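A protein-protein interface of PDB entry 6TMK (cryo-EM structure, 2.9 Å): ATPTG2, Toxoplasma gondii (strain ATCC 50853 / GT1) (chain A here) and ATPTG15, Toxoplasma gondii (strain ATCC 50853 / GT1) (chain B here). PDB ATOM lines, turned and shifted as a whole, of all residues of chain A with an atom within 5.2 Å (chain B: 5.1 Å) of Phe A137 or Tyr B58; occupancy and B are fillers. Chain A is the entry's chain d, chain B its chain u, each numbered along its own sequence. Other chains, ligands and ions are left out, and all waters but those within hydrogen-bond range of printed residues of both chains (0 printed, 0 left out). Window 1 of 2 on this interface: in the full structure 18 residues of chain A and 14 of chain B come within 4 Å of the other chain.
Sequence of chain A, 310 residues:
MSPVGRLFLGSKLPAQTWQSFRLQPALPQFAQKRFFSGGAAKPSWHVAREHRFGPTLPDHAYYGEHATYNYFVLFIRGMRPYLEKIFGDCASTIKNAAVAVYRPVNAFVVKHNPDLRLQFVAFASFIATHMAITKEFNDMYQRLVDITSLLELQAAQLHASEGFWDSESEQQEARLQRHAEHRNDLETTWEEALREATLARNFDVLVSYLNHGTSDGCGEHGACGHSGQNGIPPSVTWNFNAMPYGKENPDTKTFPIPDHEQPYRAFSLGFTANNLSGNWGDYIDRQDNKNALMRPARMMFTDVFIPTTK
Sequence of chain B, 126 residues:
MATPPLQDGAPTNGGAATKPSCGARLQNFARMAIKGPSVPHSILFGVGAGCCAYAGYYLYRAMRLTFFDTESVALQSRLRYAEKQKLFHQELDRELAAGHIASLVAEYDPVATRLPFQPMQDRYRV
Printed residues of chain A that touch a printed residue of chain B: Ile A133, Thr A134 and Phe A137.
Of the 10 printed residues of chain B, 2 touch a printed residue of chain A.
Printed residues of chain B that touch a printed residue of chain A: Tyr B54 and Tyr B58.
Along chain B the printed residues that touch a printed residue of chain A span positions 54 to 58.
O of Thr A134 lies close to OD1 of Asn A138 (2.9 Å).
OG1 of Thr A134 lies within hydrogen-bond range of OH of Tyr B54, at 2.5 Å.
Among the printed residues, pairs that only touch across the chains: Phe A137 with Tyr B58 (3.7 Å) and Ile A133 with Tyr B54 (3.7 Å).
Of the printed residues of chain A, Tyr B58 touches Phe A137.
Of the printed residues of chain B, Thr A134 touches Tyr B54.
Printed residues of chain B within 4 Å of Ile A133: Tyr B54.
Of the printed residues of chain A, Tyr B54 touches Ile A133 and Thr A134.
Tyr B57 touches none of the printed residues of chain A.
Tyr B60 touches none of the printed residues of chain A.
The nearest printed residue of chain A that does not touch Tyr B54 is Phe A137 (4.003 Å).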
ATOM      1  N   ILE A 133      19.003  -6.951 -10.661  1.00  0.00           N
ATOM      2  CA  ILE A 133      19.720  -5.683 -10.596  1.00  0.00           C
ATOM      3  C   ILE A 133      20.196  -5.273 -11.985  1.00  0.00           C
ATOM      4  O   ILE A 133      20.105  -4.094 -12.380  1.00  0.00           O
ATOM      5  CB  ILE A 133      20.884  -5.790  -9.602  1.00  0.00           C
ATOM      6  CG1 ILE A 133      20.355  -6.145  -8.219  1.00  0.00           C
ATOM      7  CG2 ILE A 133      21.626  -4.487  -9.536  1.00  0.00           C
ATOM      8  CD1 ILE A 133      21.387  -6.684  -7.307  1.00  0.00           C
ATOM      9  N   THR A 134      20.720  -6.236 -12.744  1.00  0.00           N
ATOM     10  CA  THR A 134      21.088  -5.963 -14.125  1.00  0.00           C
ATOM     11  C   THR A 134      19.895  -5.446 -14.916  1.00  0.00           C
ATOM     12  O   THR A 134      20.038  -4.542 -15.744  1.00  0.00           O
ATOM     13  CB  THR A 134      21.659  -7.224 -14.764  1.00  0.00           C
ATOM     14  OG1 THR A 134      22.566  -7.851 -13.853  1.00  0.00           O
ATOM     15  CG2 THR A 134      22.399  -6.887 -16.030  1.00  0.00           C
ATOM     16  N   LYS A 135      18.707  -5.996 -14.661  1.00  0.00           N
ATOM     17  CA  LYS A 135      17.508  -5.538 -15.352  1.00  0.00           C
ATOM     18  C   LYS A 135      17.170  -4.103 -14.986  1.00  0.00           C
ATOM     19  O   LYS A 135      16.713  -3.336 -15.835  1.00  0.00           O
ATOM     20  CB  LYS A 135      16.331  -6.452 -15.027  1.00  0.00           C
ATOM     21  CG  LYS A 135      15.140  -6.241 -15.930  1.00  0.00           C
ATOM     22  CD  LYS A 135      13.993  -7.148 -15.576  1.00  0.00           C
ATOM     23  CE  LYS A 135      12.912  -7.109 -16.639  1.00  0.00           C
ATOM     24  NZ  LYS A 135      12.557  -5.720 -17.033  1.00  0.00           N
ATOM     25  N   GLU A 136      17.373  -3.725 -13.728  1.00  0.00           N
ATOM     26  CA  GLU A 136      17.128  -2.343 -13.321  1.00  0.00           C
ATOM     27  C   GLU A 136      18.020  -1.381 -14.102  1.00  0.00           C
ATOM     28  O   GLU A 136      17.544  -0.414 -14.729  1.00  0.00           O
ATOM     29  CB  GLU A 136      17.357  -2.212 -11.816  1.00  0.00           C
ATOM     30  CG  GLU A 136      16.828  -0.936 -11.188  1.00  0.00           C
ATOM     31  CD  GLU A 136      17.883   0.147 -11.058  1.00  0.00           C
ATOM     32  OE1 GLU A 136      19.038  -0.184 -10.717  1.00  0.00           O
ATOM     33  OE2 GLU A 136      17.556   1.329 -11.296  1.00  0.00           O
ATOM     34  N   PHE A 137      19.326  -1.645 -14.088  1.00  0.00           N
ATOM     35  CA  PHE A 137      20.251  -0.793 -14.832  1.00  0.00           C
ATOM     36  C   PHE A 137      19.913  -0.768 -16.321  1.00  0.00           C
ATOM     37  O   PHE A 137      19.945   0.293 -16.967  1.00  0.00           O
ATOM     38  CB  PHE A 137      21.681  -1.277 -14.628  1.00  0.00           C
ATOM     39  CG  PHE A 137      22.240  -0.968 -13.278  1.00  0.00           C
ATOM     40  CD1 PHE A 137      22.683   0.300 -12.976  1.00  0.00           C
ATOM     41  CD2 PHE A 137      22.342  -1.948 -12.315  1.00  0.00           C
ATOM     42  CE1 PHE A 137      23.203   0.585 -11.740  1.00  0.00           C
ATOM     43  CE2 PHE A 137      22.861  -1.665 -11.080  1.00  0.00           C
ATOM     44  CZ  PHE A 137      23.292  -0.402 -10.792  1.00  0.00           C
ATOM     45  N   ASN A 138      19.591  -1.934 -16.878  1.00  0.00           N
ATOM     46  CA  ASN A 138      19.260  -2.032 -18.290  1.00  0.00           C
ATOM     47  C   ASN A 138      18.000  -1.253 -18.616  1.00  0.00           C
ATOM     48  O   ASN A 138      17.890  -0.676 -19.698  1.00  0.00           O
ATOM     49  CB  ASN A 138      19.108  -3.496 -18.677  1.00  0.00           C
ATOM     50  CG  ASN A 138      20.427  -4.206 -18.754  1.00  0.00           C
ATOM     51  OD1 ASN A 138      21.421  -3.762 -18.183  1.00  0.00           O
ATOM     52  ND2 ASN A 138      20.449  -5.318 -19.461  1.00  0.00           N
ATOM     53  N   ASP A 139      17.033  -1.234 -17.702  1.00  0.00           N
ATOM     54  CA  ASP A 139      15.814  -0.469 -17.929  1.00  0.00           C
ATOM     55  C   ASP A 139      16.127   1.014 -18.014  1.00  0.00           C
ATOM     56  O   ASP A 139      15.589   1.728 -18.871  1.00  0.00           O
ATOM     57  CB  ASP A 139      14.819  -0.751 -16.808  1.00  0.00           C
ATOM     58  CG  ASP A 139      14.206  -2.131 -16.908  1.00  0.00           C
ATOM     59  OD1 ASP A 139      14.693  -2.941 -17.723  1.00  0.00           O
ATOM     60  OD2 ASP A 139      13.236  -2.408 -16.171  1.00  0.00           O
ATOM     61  N   MET A 140      17.005   1.497 -17.138  1.00  0.00           N
ATOM     62  CA  MET A 140      17.393   2.905 -17.203  1.00  0.00           C
ATOM     63  C   MET A 140      18.055   3.241 -18.543  1.00  0.00           C
ATOM     64  O   MET A 140      17.666   4.201 -19.238  1.00  0.00           O
ATOM     65  CB  MET A 140      18.320   3.235 -16.041  1.00  0.00           C
ATOM     66  CG  MET A 140      18.310   4.691 -15.655  1.00  0.00           C
ATOM     67  SD  MET A 140      16.800   5.199 -14.832  1.00  0.00           S
ATOM     68  CE  MET A 140      17.052   6.964 -14.851  1.00  0.00           C
ATOM     69  N   TYR A 141      19.064   2.455 -18.922  1.00  0.00           N
ATOM     70  CA  TYR A 141      19.731   2.703 -20.195  1.00  0.00           C
ATOM     71  C   TYR A 141      18.768   2.566 -21.367  1.00  0.00           C
ATOM     72  O   TYR A 141      18.883   3.297 -22.359  1.00  0.00           O
ATOM     73  CB  TYR A 141      20.908   1.748 -20.346  1.00  0.00           C
ATOM     74  CG  TYR A 141      21.955   2.197 -21.330  1.00  0.00           C
ATOM     75  CD1 TYR A 141      22.851   3.195 -21.007  1.00  0.00           C
ATOM     76  CD2 TYR A 141      22.050   1.617 -22.580  1.00  0.00           C
ATOM     77  CE1 TYR A 141      23.804   3.602 -21.897  1.00  0.00           C
ATOM     78  CE2 TYR A 141      23.001   2.019 -23.474  1.00  0.00           C
ATOM     79  CZ  TYR A 141      23.879   3.008 -23.129  1.00  0.00           C
ATOM     80  OH  TYR A 141      24.832   3.407 -24.031  1.00  0.00           O
ATOM     81  N   GLN A 142      17.810   1.646 -21.269  1.00  0.00           N
ATOM     82  CA  GLN A 142      16.826   1.467 -22.322  1.00  0.00           C
ATOM     83  C   GLN A 142      15.941   2.691 -22.454  1.00  0.00           C
ATOM     84  O   GLN A 142      15.539   3.049 -23.560  1.00  0.00           O
ATOM     85  CB  GLN A 142      15.987   0.224 -22.050  1.00  0.00           C
ATOM     86  CG  GLN A 142      15.142  -0.201 -23.220  1.00  0.00           C
ATOM     87  CD  GLN A 142      15.940  -0.868 -24.310  1.00  0.00           C
ATOM     88  OE1 GLN A 142      16.624  -1.863 -24.078  1.00  0.00           O
ATOM     89  NE2 GLN A 142      15.866  -0.315 -25.513  1.00  0.00           N
ATOM     90  N   TYR B  54      27.503  -6.908  -6.476  1.00  0.00           N
ATOM     91  CA  TYR B  54      27.349  -5.587  -7.071  1.00  0.00           C
ATOM     92  C   TYR B  54      28.119  -4.523  -6.298  1.00  0.00           C
ATOM     93  O   TYR B  54      28.583  -3.545  -6.892  1.00  0.00           O
ATOM     94  CB  TYR B  54      25.871  -5.246  -7.199  1.00  0.00           C
ATOM     95  CG  TYR B  54      25.364  -5.587  -8.573  1.00  0.00           C
ATOM     96  CD1 TYR B  54      25.496  -4.694  -9.621  1.00  0.00           C
ATOM     97  CD2 TYR B  54      24.799  -6.822  -8.837  1.00  0.00           C
ATOM     98  CE1 TYR B  54      25.052  -5.009 -10.880  1.00  0.00           C
ATOM     99  CE2 TYR B  54      24.355  -7.143 -10.094  1.00  0.00           C
ATOM    100  CZ  TYR B  54      24.486  -6.235 -11.113  1.00  0.00           C
ATOM    101  OH  TYR B  54      24.044  -6.549 -12.374  1.00  0.00           O
ATOM    102  N   ALA B  55      28.290  -4.701  -4.989  1.00  0.00           N
ATOM    103  CA  ALA B  55      29.187  -3.824  -4.244  1.00  0.00           C
ATOM    104  C   ALA B  55      30.611  -3.935  -4.770  1.00  0.00           C
ATOM    105  O   ALA B  55      31.322  -2.930  -4.901  1.00  0.00           O
ATOM    106  CB  ALA B  55      29.135  -4.166  -2.760  1.00  0.00           C
ATOM    107  N   GLY B  56      31.046  -5.158  -5.068  1.00  0.00           N
ATOM    108  CA  GLY B  56      32.362  -5.340  -5.651  1.00  0.00           C
ATOM    109  C   GLY B  56      32.491  -4.669  -7.004  1.00  0.00           C
ATOM    110  O   GLY B  56      33.528  -4.084  -7.324  1.00  0.00           O
ATOM    111  N   TYR B  57      31.439  -4.752  -7.820  1.00  0.00           N
ATOM    112  CA  TYR B  57      31.451  -4.054  -9.101  1.00  0.00           C
ATOM    113  C   TYR B  57      31.559  -2.547  -8.903  1.00  0.00           C
ATOM    114  O   TYR B  57      32.296  -1.862  -9.629  1.00  0.00           O
ATOM    115  CB  TYR B  57      30.187  -4.379  -9.894  1.00  0.00           C
ATOM    116  CG  TYR B  57      30.038  -5.820 -10.308  1.00  0.00           C
ATOM    117  CD1 TYR B  57      31.129  -6.578 -10.675  1.00  0.00           C
ATOM    118  CD2 TYR B  57      28.792  -6.414 -10.348  1.00  0.00           C
ATOM    119  CE1 TYR B  57      30.985  -7.889 -11.055  1.00  0.00           C
ATOM    120  CE2 TYR B  57      28.640  -7.722 -10.725  1.00  0.00           C
ATOM    121  CZ  TYR B  57      29.737  -8.456 -11.077  1.00  0.00           C
ATOM    122  OH  TYR B  57      29.576  -9.765 -11.454  1.00  0.00           O
ATOM    123  N   TYR B  58      30.822  -2.013  -7.928  1.00  0.00           N
ATOM    124  CA  TYR B  58      30.915  -0.593  -7.614  1.00  0.00           C
ATOM    125  C   TYR B  58      32.337  -0.206  -7.237  1.00  0.00           C
ATOM    126  O   TYR B  58      32.845   0.826  -7.682  1.00  0.00           O
ATOM    127  CB  TYR B  58      29.956  -0.241  -6.481  1.00  0.00           C
ATOM    128  CG  TYR B  58      28.600   0.247  -6.932  1.00  0.00           C
ATOM    129  CD1 TYR B  58      28.405   1.562  -7.312  1.00  0.00           C
ATOM    130  CD2 TYR B  58      27.512  -0.606  -6.957  1.00  0.00           C
ATOM    131  CE1 TYR B  58      27.171   2.009  -7.714  1.00  0.00           C
ATOM    132  CE2 TYR B  58      26.273  -0.166  -7.360  1.00  0.00           C
ATOM    133  CZ  TYR B  58      26.108   1.142  -7.736  1.00  0.00           C
ATOM    134  OH  TYR B  58      24.871   1.583  -8.142  1.00  0.00           O
ATOM    135  N   LEU B  59      32.992  -1.023  -6.412  1.00  0.00           N
ATOM    136  CA  LEU B  59      34.369  -0.734  -6.016  1.00  0.00           C
ATOM    137  C   LEU B  59      35.305  -0.757  -7.218  1.00  0.00           C
ATOM    138  O   LEU B  59      36.167   0.119  -7.376  1.00  0.00           O
ATOM    139  CB  LEU B  59      34.833  -1.740  -4.968  1.00  0.00           C
ATOM    140  CG  LEU B  59      34.329  -1.496  -3.551  1.00  0.00           C
ATOM    141  CD1 LEU B  59      34.518  -2.738  -2.705  1.00  0.00           C
ATOM    142  CD2 LEU B  59      35.051  -0.317  -2.942  1.00  0.00           C
ATOM    143  N   TYR B  60      35.161  -1.777  -8.062  1.00  0.00           N
ATOM    144  CA  TYR B  60      35.983  -1.892  -9.261  1.00  0.00           C
ATOM    145  C   TYR B  60      35.872  -0.634 -10.113  1.00  0.00           C
ATOM    146  O   TYR B  60      36.886  -0.016 -10.470  1.00  0.00           O
ATOM    147  CB  TYR B  60      35.564  -3.143 -10.034  1.00  0.00           C
ATOM    148  CG  TYR B  60      36.029  -3.223 -11.462  1.00  0.00           C
ATOM    149  CD1 TYR B  60      37.371  -3.169 -11.781  1.00  0.00           C
ATOM    150  CD2 TYR B  60      35.121  -3.379 -12.492  1.00  0.00           C
ATOM    151  CE1 TYR B  60      37.795  -3.248 -13.085  1.00  0.00           C
ATOM    152  CE2 TYR B  60      35.532  -3.460 -13.797  1.00  0.00           C
ATOM    153  CZ  TYR B  60      36.871  -3.397 -14.091  1.00  0.00           C
ATOM    154  OH  TYR B  60      37.288  -3.478 -15.397  1.00  0.00           O
ATOM    155  N   ARG B  61      34.643  -0.212 -10.414  1.00  0.00           N
ATOM    156  CA  ARG B  61      34.464   0.958 -11.264  1.00  0.00           C
ATOM    157  C   ARG B  61      34.897   2.238 -10.570  1.00  0.00           C
ATOM    158  O   ARG B  61      35.420   3.144 -11.226  1.00  0.00           O
ATOM    159  CB  ARG B  61      33.009   1.074 -11.698  1.00  0.00           C
ATOM    160  CG  ARG B  61      32.484  -0.113 -12.457  1.00  0.00           C
ATOM    161  CD  ARG B  61      33.290  -0.360 -13.710  1.00  0.00           C
ATOM    162  NE  ARG B  61      33.269   0.799 -14.594  1.00  0.00           N
ATOM    163  CZ  ARG B  61      33.734   0.794 -15.836  1.00  0.00           C
ATOM    164  NH1 ARG B  61      34.253  -0.308 -16.346  1.00  0.00           N
ATOM    165  NH2 ARG B  61      33.677   1.892 -16.570  1.00  0.00           N
ATOM    166  N   ALA B  62      34.702   2.340  -9.258  1.00  0.00           N
ATOM    167  CA  ALA B  62      35.144   3.523  -8.536  1.00  0.00           C
ATOM    168  C   ALA B  62      36.648   3.693  -8.650  1.00  0.00           C
ATOM    169  O   ALA B  62      37.143   4.770  -9.010  1.00  0.00           O
ATOM    170  CB  ALA B  62      34.725   3.425  -7.073  1.00  0.00           C
ATOM    171  N   MET B  63      37.397   2.634  -8.348  1.00  0.00           N
ATOM    172  CA  MET B  63      38.849   2.725  -8.409  1.00  0.00           C
ATOM    173  C   MET B  63      39.315   2.978  -9.837  1.00  0.00           C
ATOM    174  O   MET B  63      40.234   3.776 -10.070  1.00  0.00           O
ATOM    175  CB  MET B  63      39.455   1.448  -7.834  1.00  0.00           C
ATOM    176  CG  MET B  63      40.900   1.559  -7.411  1.00  0.00           C
ATOM    177  SD  MET B  63      41.357   0.290  -6.211  1.00  0.00           S
ATOM    178  CE  MET B  63      41.247  -1.201  -7.193  1.00  0.00           C
